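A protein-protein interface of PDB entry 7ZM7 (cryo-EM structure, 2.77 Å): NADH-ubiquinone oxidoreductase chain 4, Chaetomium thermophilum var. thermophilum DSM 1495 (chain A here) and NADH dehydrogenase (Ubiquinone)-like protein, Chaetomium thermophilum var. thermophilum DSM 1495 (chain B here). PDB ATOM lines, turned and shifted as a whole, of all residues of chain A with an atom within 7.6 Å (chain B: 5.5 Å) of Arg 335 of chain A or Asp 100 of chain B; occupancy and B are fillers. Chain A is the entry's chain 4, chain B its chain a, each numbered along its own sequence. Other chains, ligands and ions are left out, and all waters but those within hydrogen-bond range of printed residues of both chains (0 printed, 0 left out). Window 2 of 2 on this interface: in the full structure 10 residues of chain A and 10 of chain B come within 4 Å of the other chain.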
ATOM      1  N   ALA A 329       9.843 -11.505 -16.614  1.00  0.00           N
ATOM      2  CA  ALA A 329      10.178 -10.343 -15.806  1.00  0.00           C
ATOM      3  C   ALA A 329      11.244 -10.678 -14.779  1.00  0.00           C
ATOM      4  O   ALA A 329      12.090  -9.841 -14.458  1.00  0.00           O
ATOM      5  CB  ALA A 329       8.932  -9.792 -15.122  1.00  0.00           C
ATOM      6  N   SER A 330      11.192 -11.884 -14.225  1.00  0.00           N
ATOM      7  CA  SER A 330      12.215 -12.313 -13.286  1.00  0.00           C
ATOM      8  C   SER A 330      13.565 -12.481 -13.968  1.00  0.00           C
ATOM      9  O   SER A 330      14.602 -12.169 -13.377  1.00  0.00           O
ATOM     10  CB  SER A 330      11.793 -13.612 -12.619  1.00  0.00           C
ATOM     11  OG  SER A 330      10.661 -13.424 -11.801  1.00  0.00           O
ATOM     12  N   PHE A 331      13.576 -12.997 -15.199  1.00  0.00           N
ATOM     13  CA  PHE A 331      14.837 -13.193 -15.911  1.00  0.00           C
ATOM     14  C   PHE A 331      15.498 -11.869 -16.245  1.00  0.00           C
ATOM     15  O   PHE A 331      16.720 -11.742 -16.152  1.00  0.00           O
ATOM     16  CB  PHE A 331      14.615 -14.000 -17.186  1.00  0.00           C
ATOM     17  CG  PHE A 331      14.165 -15.403 -16.941  1.00  0.00           C
ATOM     18  CD1 PHE A 331      14.265 -15.963 -15.683  1.00  0.00           C
ATOM     19  CD2 PHE A 331      13.623 -16.156 -17.967  1.00  0.00           C
ATOM     20  CE1 PHE A 331      13.841 -17.230 -15.458  1.00  0.00           C
ATOM     21  CE2 PHE A 331      13.196 -17.430 -17.746  1.00  0.00           C
ATOM     22  CZ  PHE A 331      13.317 -17.974 -16.490  1.00  0.00           C
ATOM     23  N   SER A 332      14.714 -10.876 -16.642  1.00  0.00           N
ATOM     24  CA  SER A 332      15.287  -9.599 -17.028  1.00  0.00           C
ATOM     25  C   SER A 332      15.443  -8.632 -15.868  1.00  0.00           C
ATOM     26  O   SER A 332      16.054  -7.578 -16.047  1.00  0.00           O
ATOM     27  CB  SER A 332      14.455  -8.966 -18.139  1.00  0.00           C
ATOM     28  OG  SER A 332      13.120  -8.815 -17.756  1.00  0.00           O
ATOM     29  N   THR A 333      14.932  -8.963 -14.689  1.00  0.00           N
ATOM     30  CA  THR A 333      15.269  -8.179 -13.513  1.00  0.00           C
ATOM     31  C   THR A 333      16.666  -8.527 -13.015  1.00  0.00           C
ATOM     32  O   THR A 333      17.267  -7.740 -12.283  1.00  0.00           O
ATOM     33  CB  THR A 333      14.216  -8.398 -12.415  1.00  0.00           C
ATOM     34  OG1 THR A 333      12.922  -8.181 -12.968  1.00  0.00           O
ATOM     35  CG2 THR A 333      14.368  -7.396 -11.291  1.00  0.00           C
ATOM     36  N   LEU A 334      17.202  -9.681 -13.409  1.00  0.00           N
ATOM     37  CA  LEU A 334      18.599  -9.994 -13.123  1.00  0.00           C
ATOM     38  C   LEU A 334      19.571  -9.121 -13.893  1.00  0.00           C
ATOM     39  O   LEU A 334      20.620  -8.760 -13.360  1.00  0.00           O
ATOM     40  CB  LEU A 334      18.901 -11.456 -13.430  1.00  0.00           C
ATOM     41  CG  LEU A 334      18.230 -12.493 -12.571  1.00  0.00           C
ATOM     42  CD1 LEU A 334      18.534 -13.861 -13.116  1.00  0.00           C
ATOM     43  CD2 LEU A 334      18.819 -12.350 -11.201  1.00  0.00           C
ATOM     44  N   ARG A 335      19.267  -8.790 -15.143  1.00  0.00           N
ATOM     45  CA  ARG A 335      20.241  -8.160 -16.020  1.00  0.00           C
ATOM     46  C   ARG A 335      20.051  -6.653 -16.143  1.00  0.00           C
ATOM     47  O   ARG A 335      20.524  -6.052 -17.106  1.00  0.00           O
ATOM     48  CB  ARG A 335      20.202  -8.827 -17.391  1.00  0.00           C
ATOM     49  CG  ARG A 335      20.611 -10.290 -17.360  1.00  0.00           C
ATOM     50  CD  ARG A 335      22.068 -10.510 -17.008  1.00  0.00           C
ATOM     51  NE  ARG A 335      22.966  -9.938 -17.998  1.00  0.00           N
ATOM     52  CZ  ARG A 335      23.264 -10.509 -19.158  1.00  0.00           C
ATOM     53  NH1 ARG A 335      22.726 -11.665 -19.485  1.00  0.00           N
ATOM     54  NH2 ARG A 335      24.088  -9.916 -20.005  1.00  0.00           N
ATOM     55  N   THR A 336      19.407  -6.027 -15.172  1.00  0.00           N
ATOM     56  CA  THR A 336      19.136  -4.598 -15.219  1.00  0.00           C
ATOM     57  C   THR A 336      20.251  -3.823 -14.525  1.00  0.00           C
ATOM     58  O   THR A 336      20.558  -4.077 -13.359  1.00  0.00           O
ATOM     59  CB  THR A 336      17.785  -4.302 -14.568  1.00  0.00           C
ATOM     60  OG1 THR A 336      16.821  -5.235 -15.054  1.00  0.00           O
ATOM     61  CG2 THR A 336      17.310  -2.904 -14.915  1.00  0.00           C
ATOM     62  N   VAL A 337      20.822  -2.846 -15.223  1.00  0.00           N
ATOM     63  CA  VAL A 337      21.991  -2.100 -14.672  1.00  0.00           C
ATOM     64  C   VAL A 337      21.531  -0.795 -14.007  1.00  0.00           C
ATOM     65  O   VAL A 337      22.362  -0.167 -13.347  1.00  0.00           O
ATOM     66  CB  VAL A 337      23.030  -1.843 -15.784  1.00  0.00           C
ATOM     67  CG1 VAL A 337      23.117  -3.010 -16.746  1.00  0.00           C
ATOM     68  CG2 VAL A 337      22.726  -0.568 -16.558  1.00  0.00           C
ATOM     69  N   ASP A 338      20.252  -0.442 -14.138  1.00  0.00           N
ATOM     70  CA  ASP A 338      19.688   0.757 -13.464  1.00  0.00           C
ATOM     71  C   ASP A 338      19.034   0.294 -12.159  1.00  0.00           C
ATOM     72  O   ASP A 338      18.181  -0.593 -12.232  1.00  0.00           O
ATOM     73  CB  ASP A 338      18.727   1.472 -14.415  1.00  0.00           C
ATOM     74  CG  ASP A 338      18.266   2.847 -13.965  1.00  0.00           C
ATOM     75  OD1 ASP A 338      17.690   2.951 -12.867  1.00  0.00           O
ATOM     76  OD2 ASP A 338      18.470   3.800 -14.735  1.00  0.00           O
ATOM     77  N   LEU A 342      15.526  -1.642 -11.762  1.00  0.00           N
ATOM     78  CA  LEU A 342      15.480  -2.998 -11.167  1.00  0.00           C
ATOM     79  C   LEU A 342      14.289  -3.093 -10.205  1.00  0.00           C
ATOM     80  O   LEU A 342      13.615  -4.126 -10.205  1.00  0.00           O
ATOM     81  CB  LEU A 342      16.823  -3.227 -10.473  1.00  0.00           C
ATOM     82  CG  LEU A 342      17.358  -4.657 -10.470  1.00  0.00           C
ATOM     83  CD1 LEU A 342      18.877  -4.655 -10.386  1.00  0.00           C
ATOM     84  CD2 LEU A 342      16.763  -5.464  -9.325  1.00  0.00           C
ATOM     85  N   TYR A 345      11.025  -3.193 -12.292  1.00  0.00           N
ATOM     86  CA  TYR A 345      10.827  -4.530 -12.898  1.00  0.00           C
ATOM     87  C   TYR A 345      10.350  -5.522 -11.840  1.00  0.00           C
ATOM     88  O   TYR A 345       9.612  -6.440 -12.196  1.00  0.00           O
ATOM     89  CB  TYR A 345      12.058  -4.938 -13.710  1.00  0.00           C
ATOM     90  CG  TYR A 345      11.732  -5.439 -15.092  1.00  0.00           C
ATOM     91  CD1 TYR A 345      10.482  -5.960 -15.375  1.00  0.00           C
ATOM     92  CD2 TYR A 345      12.661  -5.386 -16.115  1.00  0.00           C
ATOM     93  CE1 TYR A 345      10.161  -6.420 -16.638  1.00  0.00           C
ATOM     94  CE2 TYR A 345      12.356  -5.842 -17.386  1.00  0.00           C
ATOM     95  CZ  TYR A 345      11.100  -6.358 -17.648  1.00  0.00           C
ATOM     96  OH  TYR A 345      10.783  -6.815 -18.894  1.00  0.00           O
ATOM     97  N   TYR A 401      27.016  -0.083 -11.558  1.00  0.00           N
ATOM     98  CA  TYR A 401      28.459  -0.303 -11.755  1.00  0.00           C
ATOM     99  C   TYR A 401      29.227   0.619 -10.812  1.00  0.00           C
ATOM    100  O   TYR A 401      30.362   0.274 -10.466  1.00  0.00           O
ATOM    101  CB  TYR A 401      28.821   0.198 -13.150  1.00  0.00           C
ATOM    102  CG  TYR A 401      28.098  -0.449 -14.300  1.00  0.00           C
ATOM    103  CD1 TYR A 401      28.306  -1.778 -14.612  1.00  0.00           C
ATOM    104  CD2 TYR A 401      27.242   0.281 -15.106  1.00  0.00           C
ATOM    105  CE1 TYR A 401      27.661  -2.377 -15.677  1.00  0.00           C
ATOM    106  CE2 TYR A 401      26.588  -0.302 -16.177  1.00  0.00           C
ATOM    107  CZ  TYR A 401      26.797  -1.638 -16.461  1.00  0.00           C
ATOM    108  OH  TYR A 401      26.165  -2.231 -17.514  1.00  0.00           O
ATOM    109  N   TYR A 464      17.068 -12.167  -7.718  1.00  0.00           N
ATOM    110  CA  TYR A 464      17.313 -10.737  -8.033  1.00  0.00           C
ATOM    111  C   TYR A 464      17.519  -9.892  -6.776  1.00  0.00           C
ATOM    112  O   TYR A 464      18.382  -9.014  -6.823  1.00  0.00           O
ATOM    113  CB  TYR A 464      16.334 -10.151  -9.060  1.00  0.00           C
ATOM    114  CG  TYR A 464      14.853 -10.215  -8.789  1.00  0.00           C
ATOM    115  CD1 TYR A 464      14.272  -9.486  -7.767  1.00  0.00           C
ATOM    116  CD2 TYR A 464      14.016 -10.930  -9.627  1.00  0.00           C
ATOM    117  CE1 TYR A 464      12.909  -9.524  -7.540  1.00  0.00           C
ATOM    118  CE2 TYR A 464      12.650 -10.977  -9.417  1.00  0.00           C
ATOM    119  CZ  TYR A 464      12.093 -10.268  -8.371  1.00  0.00           C
ATOM    120  OH  TYR A 464      10.747 -10.312  -8.156  1.00  0.00           O
ATOM    121  N   TYR A 467      20.988 -10.438  -5.114  1.00  0.00           N
ATOM    122  CA  TYR A 467      22.076 -10.046  -6.043  1.00  0.00           C
ATOM    123  C   TYR A 467      22.209  -8.526  -6.068  1.00  0.00           C
ATOM    124  O   TYR A 467      23.343  -8.050  -5.933  1.00  0.00           O
ATOM    125  CB  TYR A 467      21.917 -10.711  -7.406  1.00  0.00           C
ATOM    126  CG  TYR A 467      23.065 -10.525  -8.363  1.00  0.00           C
ATOM    127  CD1 TYR A 467      24.379 -10.546  -7.925  1.00  0.00           C
ATOM    128  CD2 TYR A 467      22.839 -10.351  -9.718  1.00  0.00           C
ATOM    129  CE1 TYR A 467      25.436 -10.381  -8.804  1.00  0.00           C
ATOM    130  CE2 TYR A 467      23.883 -10.185 -10.610  1.00  0.00           C
ATOM    131  CZ  TYR A 467      25.186 -10.202 -10.153  1.00  0.00           C
ATOM    132  OH  TYR A 467      26.221 -10.040 -11.031  1.00  0.00           O
ATOM    133  N   ARG A 471      25.466  -6.548  -4.423  1.00  0.00           N
ATOM    134  CA  ARG A 471      26.261  -5.661  -5.296  1.00  0.00           C
ATOM    135  C   ARG A 471      26.418  -4.261  -4.693  1.00  0.00           C
ATOM    136  O   ARG A 471      27.485  -3.667  -4.887  1.00  0.00           O
ATOM    137  CB  ARG A 471      25.662  -5.640  -6.702  1.00  0.00           C
ATOM    138  CG  ARG A 471      26.118  -6.787  -7.591  1.00  0.00           C
ATOM    139  CD  ARG A 471      25.429  -6.699  -8.935  1.00  0.00           C
ATOM    140  NE  ARG A 471      23.997  -6.917  -8.822  1.00  0.00           N
ATOM    141  CZ  ARG A 471      23.137  -6.775  -9.820  1.00  0.00           C
ATOM    142  NH1 ARG A 471      21.851  -6.998  -9.625  1.00  0.00           N
ATOM    143  NH2 ARG A 471      23.567  -6.399 -11.010  1.00  0.00           N
ATOM    144  N   ARG B  72      34.392 -10.728 -25.129  1.00  0.00           N
ATOM    145  CA  ARG B  72      33.688 -11.140 -23.921  1.00  0.00           C
ATOM    146  C   ARG B  72      34.621 -12.073 -23.178  1.00  0.00           C
ATOM    147  O   ARG B  72      34.534 -13.293 -23.276  1.00  0.00           O
ATOM    148  CB  ARG B  72      32.360 -11.811 -24.253  1.00  0.00           C
ATOM    149  CG  ARG B  72      31.563 -12.192 -23.015  1.00  0.00           C
ATOM    150  CD  ARG B  72      30.251 -12.843 -23.342  1.00  0.00           C
ATOM    151  NE  ARG B  72      30.435 -14.106 -24.044  1.00  0.00           N
ATOM    152  CZ  ARG B  72      30.688 -15.262 -23.442  1.00  0.00           C
ATOM    153  NH1 ARG B  72      30.847 -16.365 -24.159  1.00  0.00           N
ATOM    154  NH2 ARG B  72      30.778 -15.316 -22.120  1.00  0.00           N
ATOM    155  N   HIS B  98      32.852  -4.555 -22.172  1.00  0.00           N
ATOM    156  CA  HIS B  98      31.876  -5.337 -22.917  1.00  0.00           C
ATOM    157  C   HIS B  98      30.477  -5.010 -22.409  1.00  0.00           C
ATOM    158  O   HIS B  98      30.275  -4.738 -21.225  1.00  0.00           O
ATOM    159  CB  HIS B  98      32.178  -6.826 -22.759  1.00  0.00           C
ATOM    160  CG  HIS B  98      31.468  -7.716 -23.733  1.00  0.00           C
ATOM    161  ND1 HIS B  98      30.116  -7.965 -23.674  1.00  0.00           N
ATOM    162  CD2 HIS B  98      31.938  -8.455 -24.762  1.00  0.00           C
ATOM    163  CE1 HIS B  98      29.777  -8.791 -24.645  1.00  0.00           C
ATOM    164  NE2 HIS B  98      30.864  -9.095 -25.326  1.00  0.00           N
ATOM    165  N   GLU B  99      29.498  -5.034 -23.312  1.00  0.00           N
ATOM    166  CA  GLU B  99      28.129  -4.733 -22.906  1.00  0.00           C
ATOM    167  C   GLU B  99      27.597  -5.723 -21.882  1.00  0.00           C
ATOM    168  O   GLU B  99      26.574  -5.458 -21.247  1.00  0.00           O
ATOM    169  CB  GLU B  99      27.201  -4.735 -24.111  1.00  0.00           C
ATOM    170  CG  GLU B  99      27.270  -6.002 -24.908  1.00  0.00           C
ATOM    171  CD  GLU B  99      26.787  -5.808 -26.315  1.00  0.00           C
ATOM    172  OE1 GLU B  99      26.249  -4.722 -26.608  1.00  0.00           O
ATOM    173  OE2 GLU B  99      26.945  -6.738 -27.133  1.00  0.00           O
ATOM    174  N   ASP B 100      28.246  -6.874 -21.736  1.00  0.00           N
ATOM    175  CA  ASP B 100      27.873  -7.861 -20.740  1.00  0.00           C
ATOM    176  C   ASP B 100      28.624  -7.648 -19.439  1.00  0.00           C
ATOM    177  O   ASP B 100      28.853  -8.595 -18.687  1.00  0.00           O
ATOM    178  CB  ASP B 100      28.115  -9.264 -21.277  1.00  0.00           C
ATOM    179  CG  ASP B 100      26.991  -9.751 -22.150  1.00  0.00           C
ATOM    180  OD1 ASP B 100      25.824  -9.430 -21.858  1.00  0.00           O
ATOM    181  OD2 ASP B 100      27.271 -10.477 -23.121  1.00  0.00           O
ATOM    182  N   HIS B 101      29.054  -6.406 -19.206  1.00  0.00           N
ATOM    183  CA  HIS B 101      29.872  -6.070 -18.010  1.00  0.00           C
ATOM    184  C   HIS B 101      29.262  -6.627 -16.718  1.00  0.00           C
ATOM    185  O   HIS B 101      30.052  -7.032 -15.848  1.00  0.00           O
ATOM    186  CB  HIS B 101      30.100  -4.552 -17.969  1.00  0.00           C
ATOM    187  CG  HIS B 101      31.093  -4.088 -16.959  1.00  0.00           C
ATOM    188  ND1 HIS B 101      32.446  -4.076 -17.211  1.00  0.00           N
ATOM    189  CD2 HIS B 101      30.937  -3.596 -15.712  1.00  0.00           C
ATOM    190  CE1 HIS B 101      33.083  -3.599 -16.161  1.00  0.00           C
ATOM    191  NE2 HIS B 101      32.179  -3.300 -15.227  1.00  0.00           N
ATOM    192  N   ASP B 102      27.930  -6.651 -16.592  1.00  0.00           N
ATOM    193  CA  ASP B 102      27.327  -7.091 -15.337  1.00  0.00           C
ATOM    194  C   ASP B 102      27.882  -8.435 -14.904  1.00  0.00           C
ATOM    195  O   ASP B 102      28.202  -8.643 -13.731  1.00  0.00           O
ATOM    196  CB  ASP B 102      25.811  -7.209 -15.480  1.00  0.00           C
ATOM    197  CG  ASP B 102      25.144  -5.898 -15.736  1.00  0.00           C
ATOM    198  OD1 ASP B 102      25.768  -4.850 -15.476  1.00  0.00           O
ATOM    199  OD2 ASP B 102      23.989  -5.916 -16.206  1.00  0.00           O
ATOM    200  N   ILE B 103      27.988  -9.364 -15.838  1.00  0.00           N
ATOM    201  CA  ILE B 103      28.232 -10.757 -15.530  1.00  0.00           C
ATOM    202  C   ILE B 103      29.583 -11.221 -16.060  1.00  0.00           C
ATOM    203  O   ILE B 103      29.779 -12.403 -16.296  1.00  0.00           O
ATOM    204  CB  ILE B 103      27.086 -11.631 -16.054  1.00  0.00           C
ATOM    205  CG1 ILE B 103      26.838 -11.348 -17.533  1.00  0.00           C
ATOM    206  CG2 ILE B 103      25.840 -11.331 -15.280  1.00  0.00           C
ATOM    207  CD1 ILE B 103      26.067 -12.440 -18.238  1.00  0.00           C
ATOM    208  N   LEU B 104      30.504 -10.290 -16.277  1.00  0.00           N
ATOM    209  CA  LEU B 104      31.881 -10.595 -16.616  1.00  0.00           C
ATOM    210  C   LEU B 104      32.828 -10.244 -15.486  1.00  0.00           C
ATOM    211  O   LEU B 104      34.033 -10.477 -15.606  1.00  0.00           O
ATOM    212  CB  LEU B 104      32.304  -9.839 -17.868  1.00  0.00           C
ATOM    213  CG  LEU B 104      31.867 -10.293 -19.254  1.00  0.00           C
ATOM    214  CD1 LEU B 104      32.234  -9.222 -20.252  1.00  0.00           C
ATOM    215  CD2 LEU B 104      32.518 -11.579 -19.628  1.00  0.00           C
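Thr 333 of chain A touches none of the printed residues of chain B.
Arg 335 of chain A touches just these residues of chain B: Asp 100, Asp 102 and Ile 103.
Printed residues of chain B within 4 Å of Tyr 467 of chain A: Asp 102 (3.6 Å).
Of chain A, only Arg 335 comes within 4 Å of Asp 100 of chain B.
Of the printed residues of chain A, His 101 of chain B touches Tyr 401.
Printed residues of chain A within 4 Å of Asp 102 of chain B: Arg 335, Val 337, Tyr 401 and Tyr 467.
Printed residues of chain A within 4 Å of Ile 103 of chain B: Arg 335.
The nearest printed residue of chain A that does not touch His 101 of chain B is Arg 335 of chain A (6.1 Å).
Arg 335 of chain A touches Asp 102 of chain B (O to OD2, 3.6 Å).
CD1 of Ile 103 of chain B touches CZ of Arg 335 of chain A (3.5 Å).
CG1 of Val 337 of chain A touches OD2 of Asp 102 of chain B, 3.1 Å away.
CD1 of Tyr 401 of chain A touches CD2 of His 101 of chain B, at 3.4 Å.
Tyr 467 of chain A touches Asp 102 of chain B (OH to O, 3.6 Å).
A ring nitrogen (ND1) of His 98 of chain B sits at hydrogen-bond distance from the backbone NH (N) of Asp 100 of chain B, 2.9 Å away.
The backbone carbonyl oxygen (O) of Tyr 467 of chain A is in hydrogen-bond range of the guanidinium group (NE) of Arg 471 of chain A.
The side-chain carboxylate (OD1) of Asp 100 of chain B is in salt-bridge range of the guanidinium group (NH2) of Arg 335 of chain A (2.6 Å).
The side-chain hydroxyl of Tyr 401 of chain A sits close to the side-chain carboxylate of Asp 102 of chain B, at 3.3 Å.
Of the 16 printed residues of chain A, 4 touch a printed residue of chain B.
Printed residues of chain A that touch a printed residue of chain B: Arg 335, Val 337, Tyr 401 and Tyr 467.
Hydrophobic or aromatic side chains of chain A within 4 Å of the printed part of chain B: Val 337, Tyr 401 and Tyr 467.
Printed residues of chain B that touch a printed residue of chain A: Asp 100, His 101, Asp 102 and Ile 103.
Among the printed residues, 7 pairs touch across the chains.
Among the printed residues, Asp or Glu carboxylates within 4 Å of a Lys or Arg side-chain nitrogen of the other chain: Arg 335 of chain A with Asp 100 of chain B (2.6 Å).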
